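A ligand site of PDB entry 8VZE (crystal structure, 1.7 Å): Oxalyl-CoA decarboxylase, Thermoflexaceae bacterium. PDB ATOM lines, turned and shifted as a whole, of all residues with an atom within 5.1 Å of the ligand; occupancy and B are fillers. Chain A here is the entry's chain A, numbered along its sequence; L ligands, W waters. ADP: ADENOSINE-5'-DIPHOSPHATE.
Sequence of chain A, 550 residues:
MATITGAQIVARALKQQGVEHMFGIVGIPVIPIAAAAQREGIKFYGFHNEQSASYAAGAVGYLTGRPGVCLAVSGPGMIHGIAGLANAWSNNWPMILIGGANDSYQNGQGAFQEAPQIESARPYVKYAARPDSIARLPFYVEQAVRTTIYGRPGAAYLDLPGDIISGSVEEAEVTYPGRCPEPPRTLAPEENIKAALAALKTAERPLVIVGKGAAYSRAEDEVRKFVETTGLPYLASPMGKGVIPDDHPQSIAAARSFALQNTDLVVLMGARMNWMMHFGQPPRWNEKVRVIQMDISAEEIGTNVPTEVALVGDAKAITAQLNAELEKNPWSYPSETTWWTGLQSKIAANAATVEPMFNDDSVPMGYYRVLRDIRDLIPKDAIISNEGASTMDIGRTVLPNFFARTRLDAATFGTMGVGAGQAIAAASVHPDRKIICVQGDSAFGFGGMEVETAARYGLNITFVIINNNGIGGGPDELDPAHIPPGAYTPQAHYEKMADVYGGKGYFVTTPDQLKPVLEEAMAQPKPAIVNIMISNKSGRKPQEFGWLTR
NE of Arg 152 sits close to ND2 of Asn 92, 3.4 Å away. The backbone NH (N) of Ala 315 lies within hydrogen-bond range of the side-chain hydroxyl (OG) of Ser 217 (3.5 Å). The side-chain hydroxyl (OG1) of Thr 412 is in hydrogen-bond range of the guanidinium group (NH2) of Arg 272. The side-chain carboxylate (OD1) of Asp 295 lies within hydrogen-bond range of the backbone NH (N) of Ser 297. The side-chain amide oxygen of Asn 91 sits at hydrogen-bond distance from the side-chain amino group of Lys 212 (2.9 Å). The backbone NH of Lys 212 is in hydrogen-bond range of the backbone carbonyl oxygen of Gly 270, at 3.5 Å. The backbone NH (N) of Met 276 sits close to the side-chain amide oxygen (OD1) of Asn 274, at 3.1 Å. NH2 of Arg 152 is in salt-bridge range of OE1 of Glu 300 (3.0 Å).
N of Lys 212 sits at hydrogen-bond distance from O2B of the ligand. OD1 of Asp 314 sits at hydrogen-bond distance from N6 of the ligand (2.9 Å). N of Ile 296 lies within hydrogen-bond range of N3 of the ligand, 3.2 Å away. An oxygen (O1A) of the ligand is in salt-bridge range of the side-chain amino group (NZ) of Lys 212 (2.8 Å). The side-chain hydroxyl (OG) of Ser 237 is in hydrogen-bond range of an oxygen (O2B) of the ligand (2.6 Å). The backbone NH (N) of Ala 315 sits at hydrogen-bond distance from a nitrogen (N1) of the ligand. The guanidinium group (NE) of Arg 272 lies within salt-bridge range of an oxygen (O2A) of the ligand (2.8 Å). The guanidinium group (NE) of Arg 152 is in hydrogen-bond range of an oxygen (O2') of the ligand (2.9 Å). O2A of the ligand lies close to N of Arg 272 (3.4 Å). OD2 of Asp 295 is in hydrogen-bond range of O3' of the ligand.
SD of Met 276 lies close to O1B of the ligand, at 3.4 Å. OD1 of Asn 92 touches C3' of the ligand (3.9 Å). Gly 211 touches the ligand. Gly 213 touches the ligand. Tyr 216 touches the ligand (CD2 to N7, 3.6 Å). Ser 217 touches the ligand. O of Gly 270 touches C5' of the ligand, at 3.4 Å. CB of Ala 271 touches O3B of the ligand, 3.6 Å away. ND2 of Asn 274 touches O2A of the ligand, 3.8 Å away. CB of Ser 297 touches O2' of the ligand (3.9 Å). O of Gly 313 touches C2 of the ligand, at 3.5 Å. OG1 of Thr 412 touches O1A of the ligand, at 3.6 Å. Hydrophobic or aromatic side chains that line the ligand: Tyr 216, Ala 271, Met 276, Ile 296 and Ala 315. 20 residues have an atom within 4 Å of the ligand: Asn 92, Arg 152, Gly 211, Lys 212, Gly 213, Tyr 216, Ser 217, Ser 237, Gly 270, Ala 271, Arg 272, Asn 274, Met 276, Asp 295, Ile 296, Ser 297, Gly 313, Asp 314, Ala 315 and Thr 412. Along chain A the residues within 4 Å of the ligand span positions 92 to 412. The nearest printed residue that does not touch the ligand is Glu 300 (4.1 Å).
Water W1 lies within hydrogen-bond range of an oxygen (O3B) of the ligand (2.5 Å), the side-chain amide oxygen of Asn 274 (2.9 Å) and the backbone carbonyl oxygen of Arg 272 (2.9 Å). Water W6 lies within hydrogen-bond range of O2A of the ligand (2.7 Å), OG1 of Thr 412 (2.8 Å), ND2 of Asn 274 (2.9 Å) and SD of Met 276 (3.5 Å). Water W3 lies within hydrogen-bond range of the backbone carbonyl oxygen (O) of Asn 91, an oxygen (O1A) of the ligand and the side-chain amide oxygen (OD1) of Asn 92. Water W4 lies within hydrogen-bond range of an oxygen (O1B) of the ligand (2.9 Å) and the backbone NH of Met 239 (3.0 Å). Water W2 lies within hydrogen-bond range of the backbone carbonyl oxygen (O) of Asn 92 (2.7 Å) and a nitrogen (N7) of the ligand (3.5 Å).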
ATOM      1  N   ASN A  91      16.367 -18.889  29.585  1.00  0.00           N
ATOM      2  CA  ASN A  91      15.570 -17.680  29.769  1.00  0.00           C
ATOM      3  C   ASN A  91      16.308 -16.410  29.397  1.00  0.00           C
ATOM      4  O   ASN A  91      15.711 -15.335  29.468  1.00  0.00           O
ATOM      5  CB  ASN A  91      15.112 -17.565  31.227  1.00  0.00           C
ATOM      6  CG  ASN A  91      14.051 -18.575  31.563  1.00  0.00           C
ATOM      7  OD1 ASN A  91      12.938 -18.503  31.035  1.00  0.00           O
ATOM      8  ND2 ASN A  91      14.385 -19.516  32.444  1.00  0.00           N
ATOM      9  N   ASN A  92      17.580 -16.510  28.957  1.00  0.00           N
ATOM     10  CA  ASN A  92      18.413 -15.323  28.693  1.00  0.00           C
ATOM     11  C   ASN A  92      18.440 -14.376  29.901  1.00  0.00           C
ATOM     12  O   ASN A  92      18.164 -13.176  29.797  1.00  0.00           O
ATOM     13  CB  ASN A  92      17.926 -14.558  27.449  1.00  0.00           C
ATOM     14  CG  ASN A  92      17.762 -15.478  26.233  1.00  0.00           C
ATOM     15  OD1 ASN A  92      16.636 -15.716  25.778  1.00  0.00           O
ATOM     16  ND2 ASN A  92      18.858 -16.003  25.728  1.00  0.00           N
ATOM     17  N   ARG A 152      22.385 -10.178  24.202  1.00  0.00           N
ATOM     18  CA  ARG A 152      21.330 -11.036  24.730  1.00  0.00           C
ATOM     19  C   ARG A 152      21.826 -11.581  26.075  1.00  0.00           C
ATOM     20  O   ARG A 152      22.858 -12.254  26.111  1.00  0.00           O
ATOM     21  CB  ARG A 152      21.037 -12.189  23.767  1.00  0.00           C
ATOM     22  CG  ARG A 152      19.711 -12.895  24.072  1.00  0.00           C
ATOM     23  CD  ARG A 152      19.476 -14.071  23.123  1.00  0.00           C
ATOM     24  NE  ARG A 152      18.060 -14.316  22.931  1.00  0.00           N
ATOM     25  CZ  ARG A 152      17.579 -15.299  22.174  1.00  0.00           C
ATOM     26  NH1 ARG A 152      18.391 -16.180  21.606  1.00  0.00           N
ATOM     27  NH2 ARG A 152      16.269 -15.402  22.012  1.00  0.00           N
ATOM     28  N   PRO A 153      21.148 -11.265  27.190  1.00  0.00           N
ATOM     29  CA  PRO A 153      21.719 -11.608  28.499  1.00  0.00           C
ATOM     30  C   PRO A 153      21.813 -13.121  28.696  1.00  0.00           C
ATOM     31  O   PRO A 153      21.053 -13.908  28.124  1.00  0.00           O
ATOM     32  CB  PRO A 153      20.748 -10.954  29.493  1.00  0.00           C
ATOM     33  CG  PRO A 153      20.053  -9.836  28.728  1.00  0.00           C
ATOM     34  CD  PRO A 153      19.960 -10.406  27.300  1.00  0.00           C
ATOM     35  N   GLY A 211       5.812  -9.970  26.486  1.00  0.00           N
ATOM     36  CA  GLY A 211       6.583 -11.047  27.086  1.00  0.00           C
ATOM     37  C   GLY A 211       7.585 -10.580  28.132  1.00  0.00           C
ATOM     38  O   GLY A 211       7.727  -9.387  28.417  1.00  0.00           O
ATOM     39  N   LYS A 212       8.322 -11.548  28.691  1.00  0.00           N
ATOM     40  CA  LYS A 212       9.203 -11.219  29.794  1.00  0.00           C
ATOM     41  C   LYS A 212      10.473 -10.535  29.318  1.00  0.00           C
ATOM     42  O   LYS A 212      11.230 -10.040  30.164  1.00  0.00           O
ATOM     43  CB  LYS A 212       9.548 -12.442  30.656  1.00  0.00           C
ATOM     44  CG  LYS A 212      10.485 -13.498  30.055  1.00  0.00           C
ATOM     45  CD  LYS A 212      10.797 -14.580  31.118  1.00  0.00           C
ATOM     46  CE  LYS A 212      11.892 -15.562  30.614  1.00  0.00           C
ATOM     47  NZ  LYS A 212      11.227 -16.616  29.744  1.00  0.00           N
ATOM     48  N   GLY A 213      10.704 -10.482  28.004  1.00  0.00           N
ATOM     49  CA  GLY A 213      11.750  -9.594  27.495  1.00  0.00           C
ATOM     50  C   GLY A 213      11.402  -8.126  27.692  1.00  0.00           C
ATOM     51  O   GLY A 213      12.270  -7.300  27.989  1.00  0.00           O
ATOM     52  N   TYR A 216      12.026  -7.615  31.357  1.00  0.00           N
ATOM     53  CA  TYR A 216      13.444  -7.536  31.675  1.00  0.00           C
ATOM     54  C   TYR A 216      14.018  -6.182  31.281  1.00  0.00           C
ATOM     55  O   TYR A 216      14.850  -5.601  32.000  1.00  0.00           O
ATOM     56  CB  TYR A 216      14.207  -8.666  30.965  1.00  0.00           C
ATOM     57  CG  TYR A 216      15.683  -8.551  31.240  1.00  0.00           C
ATOM     58  CD1 TYR A 216      16.202  -9.041  32.434  1.00  0.00           C
ATOM     59  CD2 TYR A 216      16.539  -7.909  30.350  1.00  0.00           C
ATOM     60  CE1 TYR A 216      17.542  -8.918  32.727  1.00  0.00           C
ATOM     61  CE2 TYR A 216      17.896  -7.767  30.631  1.00  0.00           C
ATOM     62  CZ  TYR A 216      18.381  -8.281  31.837  1.00  0.00           C
ATOM     63  OH  TYR A 216      19.724  -8.144  32.156  1.00  0.00           O
ATOM     64  N   SER A 217      13.594  -5.659  30.127  1.00  0.00           N
ATOM     65  CA  SER A 217      14.053  -4.359  29.629  1.00  0.00           C
ATOM     66  C   SER A 217      13.570  -3.187  30.481  1.00  0.00           C
ATOM     67  O   SER A 217      14.074  -2.058  30.318  1.00  0.00           O
ATOM     68  CB  SER A 217      13.571  -4.225  28.177  1.00  0.00           C
ATOM     69  OG  SER A 217      13.952  -2.997  27.562  1.00  0.00           O
ATOM     70  N   SER A 237       2.295 -12.930  28.165  1.00  0.00           N
ATOM     71  CA  SER A 237       2.877 -14.235  28.435  1.00  0.00           C
ATOM     72  C   SER A 237       2.868 -14.479  29.937  1.00  0.00           C
ATOM     73  O   SER A 237       2.600 -13.570  30.729  1.00  0.00           O
ATOM     74  CB  SER A 237       4.288 -14.294  27.874  1.00  0.00           C
ATOM     75  OG  SER A 237       5.125 -13.597  28.796  1.00  0.00           O
ATOM     76  N   MET A 239       5.201 -14.854  32.346  1.00  0.00           N
ATOM     77  CA  MET A 239       5.966 -13.910  33.135  1.00  0.00           C
ATOM     78  C   MET A 239       5.927 -12.504  32.547  1.00  0.00           C
ATOM     79  O   MET A 239       6.460 -11.585  33.154  1.00  0.00           O
ATOM     80  CB  MET A 239       7.405 -14.412  33.319  1.00  0.00           C
ATOM     81  CG  MET A 239       7.470 -15.493  34.445  1.00  0.00           C
ATOM     82  SD  MET A 239       9.099 -16.139  34.764  1.00  0.00           S
ATOM     83  CE  MET A 239       9.913 -14.653  35.345  1.00  0.00           C
ATOM     84  N   GLY A 240       5.233 -12.314  31.426  1.00  0.00           N
ATOM     85  CA  GLY A 240       4.874 -10.944  31.044  1.00  0.00           C
ATOM     86  C   GLY A 240       3.683 -10.359  31.802  1.00  0.00           C
ATOM     87  O   GLY A 240       3.433  -9.147  31.666  1.00  0.00           O
ATOM     88  N   GLY A 270       9.125  -8.534  23.017  1.00  0.00           N
ATOM     89  CA  GLY A 270       9.987  -9.327  23.861  1.00  0.00           C
ATOM     90  C   GLY A 270       9.400 -10.681  24.234  1.00  0.00           C
ATOM     91  O   GLY A 270       9.348 -11.008  25.415  1.00  0.00           O
ATOM     92  N   ALA A 271       8.948 -11.446  23.243  1.00  0.00           N
ATOM     93  CA  ALA A 271       8.377 -12.781  23.448  1.00  0.00           C
ATOM     94  C   ALA A 271       8.769 -13.646  22.259  1.00  0.00           C
ATOM     95  O   ALA A 271       8.798 -13.159  21.120  1.00  0.00           O
ATOM     96  CB  ALA A 271       6.847 -12.707  23.544  1.00  0.00           C
ATOM     97  N   ARG A 272       9.091 -14.924  22.512  1.00  0.00           N
ATOM     98  CA  ARG A 272       9.553 -15.783  21.420  1.00  0.00           C
ATOM     99  C   ARG A 272       8.420 -16.591  20.825  1.00  0.00           C
ATOM    100  O   ARG A 272       7.484 -16.988  21.515  1.00  0.00           O
ATOM    101  CB  ARG A 272      10.657 -16.734  21.865  1.00  0.00           C
ATOM    102  CG  ARG A 272      11.967 -16.030  22.104  1.00  0.00           C
ATOM    103  CD  ARG A 272      13.009 -16.985  22.603  1.00  0.00           C
ATOM    104  NE  ARG A 272      12.786 -17.316  24.005  1.00  0.00           N
ATOM    105  CZ  ARG A 272      13.721 -17.870  24.765  1.00  0.00           C
ATOM    106  NH1 ARG A 272      14.849 -18.312  24.237  1.00  0.00           N
ATOM    107  NH2 ARG A 272      13.547 -17.924  26.093  1.00  0.00           N
ATOM    108  N   ASN A 274       8.333 -19.632  20.454  1.00  0.00           N
ATOM    109  CA  ASN A 274       8.842 -20.942  20.831  1.00  0.00           C
ATOM    110  C   ASN A 274       7.665 -21.808  21.301  1.00  0.00           C
ATOM    111  O   ASN A 274       6.515 -21.528  20.975  1.00  0.00           O
ATOM    112  CB  ASN A 274       9.959 -20.790  21.891  1.00  0.00           C
ATOM    113  CG  ASN A 274       9.448 -20.252  23.225  1.00  0.00           C
ATOM    114  OD1 ASN A 274       8.294 -19.879  23.359  1.00  0.00           O
ATOM    115  ND2 ASN A 274      10.342 -20.187  24.240  1.00  0.00           N
ATOM    116  N   MET A 276       6.098 -22.038  23.915  1.00  0.00           N
ATOM    117  CA  MET A 276       5.080 -21.378  24.745  1.00  0.00           C
ATOM    118  C   MET A 276       4.029 -20.733  23.875  1.00  0.00           C
ATOM    119  O   MET A 276       2.858 -20.612  24.275  1.00  0.00           O
ATOM    120  CB  MET A 276       5.743 -20.302  25.615  1.00  0.00           C
ATOM    121  CG  MET A 276       5.246 -20.239  27.033  1.00  0.00           C
ATOM    122  SD  MET A 276       6.343 -19.232  28.060  1.00  0.00           S
ATOM    123  CE  MET A 276       7.344 -20.477  28.831  1.00  0.00           C
ATOM    124  N   MET A 277       4.412 -20.306  22.682  1.00  0.00           N
ATOM    125  CA  MET A 277       3.503 -19.709  21.736  1.00  0.00           C
ATOM    126  C   MET A 277       3.192 -20.676  20.589  1.00  0.00           C
ATOM    127  O   MET A 277       2.791 -20.245  19.507  1.00  0.00           O
ATOM    128  CB  MET A 277       4.097 -18.399  21.196  1.00  0.00           C
ATOM    129  CG  MET A 277       4.313 -17.332  22.248  1.00  0.00           C
ATOM    130  SD  MET A 277       2.750 -16.736  22.949  1.00  0.00           S
ATOM    131  CE  MET A 277       3.214 -16.181  24.614  1.00  0.00           C
ATOM    132  N   MET A 294       9.826  -7.675  18.053  1.00  0.00           N
ATOM    133  CA  MET A 294      10.722  -6.780  18.782  1.00  0.00           C
ATOM    134  C   MET A 294      11.557  -7.624  19.727  1.00  0.00           C
ATOM    135  O   MET A 294      11.034  -8.230  20.673  1.00  0.00           O
ATOM    136  CB  MET A 294       9.896  -5.712  19.519  1.00  0.00           C
ATOM    137  CG  MET A 294      10.719  -4.796  20.417  1.00  0.00           C
ATOM    138  SD  MET A 294       9.650  -3.803  21.530  1.00  0.00           S
ATOM    139  CE  MET A 294       8.564  -2.989  20.367  1.00  0.00           C
ATOM    140  N   ASP A 295      12.861  -7.687  19.467  1.00  0.00           N
ATOM    141  CA  ASP A 295      13.774  -8.512  20.248  1.00  0.00           C
ATOM    142  C   ASP A 295      15.174  -7.914  20.204  1.00  0.00           C
ATOM    143  O   ASP A 295      15.593  -7.373  19.185  1.00  0.00           O
ATOM    144  CB  ASP A 295      13.780  -9.959  19.713  1.00  0.00           C
ATOM    145  CG  ASP A 295      14.194 -10.981  20.788  1.00  0.00           C
ATOM    146  OD1 ASP A 295      15.344 -10.911  21.311  1.00  0.00           O
ATOM    147  OD2 ASP A 295      13.340 -11.847  21.138  1.00  0.00           O
ATOM    148  N   ILE A 296      15.900  -8.040  21.326  1.00  0.00           N
ATOM    149  CA  ILE A 296      17.293  -7.585  21.380  1.00  0.00           C
ATOM    150  C   ILE A 296      18.200  -8.495  20.561  1.00  0.00           C
ATOM    151  O   ILE A 296      19.293  -8.070  20.134  1.00  0.00           O
ATOM    152  CB  ILE A 296      17.740  -7.493  22.843  1.00  0.00           C
ATOM    153  CG1 ILE A 296      18.981  -6.588  22.949  1.00  0.00           C
ATOM    154  CG2 ILE A 296      18.009  -8.923  23.439  1.00  0.00           C
ATOM    155  CD1 ILE A 296      19.379  -6.261  24.414  1.00  0.00           C
ATOM    156  N   SER A 297      17.760  -9.740  20.314  1.00  0.00           N
ATOM    157  CA  SER A 297      18.570 -10.755  19.642  1.00  0.00           C
ATOM    158  C   SER A 297      18.222 -10.800  18.163  1.00  0.00           C
ATOM    159  O   SER A 297      17.141 -11.264  17.800  1.00  0.00           O
ATOM    160  CB  SER A 297      18.337 -12.121  20.301  1.00  0.00           C
ATOM    161  OG  SER A 297      19.032 -13.144  19.599  1.00  0.00           O
ATOM    162  N   GLU A 300      17.216 -14.266  16.768  1.00  0.00           N
ATOM    163  CA  GLU A 300      15.881 -14.802  17.063  1.00  0.00           C
ATOM    164  C   GLU A 300      14.838 -14.402  16.006  1.00  0.00           C
ATOM    165  O   GLU A 300      13.815 -15.095  15.852  1.00  0.00           O
ATOM    166  CB  GLU A 300      15.456 -14.330  18.451  1.00  0.00           C
ATOM    167  CG  GLU A 300      14.117 -14.884  18.936  1.00  0.00           C
ATOM    168  CD  GLU A 300      14.165 -16.383  19.175  1.00  0.00           C
ATOM    169  OE1 GLU A 300      15.236 -16.861  19.608  1.00  0.00           O
ATOM    170  OE2 GLU A 300      13.131 -17.055  18.918  1.00  0.00           O
ATOM    171  N   GLY A 313      16.628  -4.496  18.907  1.00  0.00           N
ATOM    172  CA  GLY A 313      17.176  -3.540  19.840  1.00  0.00           C
ATOM    173  C   GLY A 313      16.513  -3.716  21.182  1.00  0.00           C
ATOM    174  O   GLY A 313      15.902  -4.745  21.471  1.00  0.00           O
ATOM    175  N   ASP A 314      16.632  -2.682  21.998  1.00  0.00           N
ATOM    176  CA  ASP A 314      16.084  -2.748  23.351  1.00  0.00           C
ATOM    177  C   ASP A 314      14.589  -2.416  23.338  1.00  0.00           C
ATOM    178  O   ASP A 314      14.151  -1.460  22.690  1.00  0.00           O
ATOM    179  CB  ASP A 314      16.836  -1.787  24.253  1.00  0.00           C
ATOM    180  CG  ASP A 314      16.226  -1.705  25.619  1.00  0.00           C
ATOM    181  OD1 ASP A 314      16.375  -2.672  26.385  1.00  0.00           O
ATOM    182  OD2 ASP A 314      15.601  -0.659  25.911  1.00  0.00           O
ATOM    183  N   ALA A 315      13.796  -3.206  24.095  1.00  0.00           N
ATOM    184  CA  ALA A 315      12.342  -3.037  24.029  1.00  0.00           C
ATOM    185  C   ALA A 315      11.904  -1.669  24.547  1.00  0.00           C
ATOM    186  O   ALA A 315      10.978  -1.056  24.000  1.00  0.00           O
ATOM    187  CB  ALA A 315      11.645  -4.130  24.859  1.00  0.00           C
ATOM    188  N   THR A 412      10.934 -20.591  30.771  1.00  0.00           N
ATOM    189  CA  THR A 412      11.059 -21.195  29.439  1.00  0.00           C
ATOM    190  C   THR A 412      11.470 -22.655  29.490  1.00  0.00           C
ATOM    191  O   THR A 412      11.085 -23.439  28.603  1.00  0.00           O
ATOM    192  CB  THR A 412      12.065 -20.417  28.585  1.00  0.00           C
ATOM    193  OG1 THR A 412      11.582 -19.083  28.444  1.00  0.00           O
ATOM    194  CG2 THR A 412      12.160 -21.055  27.172  1.00  0.00           C
HETATM  195  PB  ADP L   1       8.092 -15.207  27.170  1.00  0.00           P
HETATM  196  O1B ADP L   1       8.428 -16.498  27.890  1.00  0.00           O
HETATM  197  O2B ADP L   1       7.593 -14.112  28.044  1.00  0.00           O
HETATM  198  O3B ADP L   1       7.300 -15.341  25.883  1.00  0.00           O
HETATM  199  PA  ADP L   1      10.788 -15.402  26.080  1.00  0.00           P
HETATM  200  O1A ADP L   1      11.750 -15.686  27.173  1.00  0.00           O
HETATM  201  O2A ADP L   1      10.337 -16.526  25.205  1.00  0.00           O
HETATM  202  O3A ADP L   1       9.509 -14.584  26.657  1.00  0.00           O
HETATM  203  O5' ADP L   1      11.376 -14.258  25.118  1.00  0.00           O
HETATM  204  C5' ADP L   1      11.966 -13.088  25.655  1.00  0.00           C
HETATM  205  C4' ADP L   1      12.748 -12.441  24.522  1.00  0.00           C
HETATM  206  O4' ADP L   1      13.128 -11.147  25.020  1.00  0.00           O
HETATM  207  C3' ADP L   1      14.042 -13.231  24.222  1.00  0.00           C
HETATM  208  O3' ADP L   1      14.077 -13.685  22.849  1.00  0.00           O
HETATM  209  C2' ADP L   1      15.165 -12.226  24.507  1.00  0.00           C
HETATM  210  O2' ADP L   1      16.202 -12.163  23.519  1.00  0.00           O
HETATM  211  C1' ADP L   1      14.420 -10.892  24.491  1.00  0.00           C
HETATM  212  N9  ADP L   1      15.067  -9.844  25.324  1.00  0.00           N
HETATM  213  C8  ADP L   1      15.842  -9.957  26.420  1.00  0.00           C
HETATM  214  N7  ADP L   1      16.223  -8.708  26.843  1.00  0.00           N
HETATM  215  C5  ADP L   1      15.668  -7.813  26.005  1.00  0.00           C
HETATM  216  C6  ADP L   1      15.656  -6.357  25.837  1.00  0.00           C
HETATM  217  N6  ADP L   1      16.327  -5.590  26.710  1.00  0.00           N
HETATM  218  N1  ADP L   1      14.937  -5.827  24.823  1.00  0.00           N
HETATM  219  C2  ADP L   1      14.272  -6.594  23.941  1.00  0.00           C
HETATM  220  N3  ADP L   1      14.256  -7.944  24.036  1.00  0.00           N
HETATM  221  C4  ADP L   1      14.915  -8.568  25.029  1.00  0.00           C
HETATM  222  O   HOH W   1       7.321 -17.360  24.391  1.00  0.00           O
HETATM  223  O   HOH W   2      16.369 -11.273  29.149  1.00  0.00           O
HETATM  224  O   HOH W   3      14.275 -14.652  27.340  1.00  0.00           O
HETATM  225  O   HOH W   4       6.916 -16.281  30.393  1.00  0.00           O
HETATM  226  O   HOH W   5      19.194  -5.568  28.170  1.00  0.00           O
HETATM  227  O   HOH W   6       9.534 -18.711  26.613  1.00  0.00           O
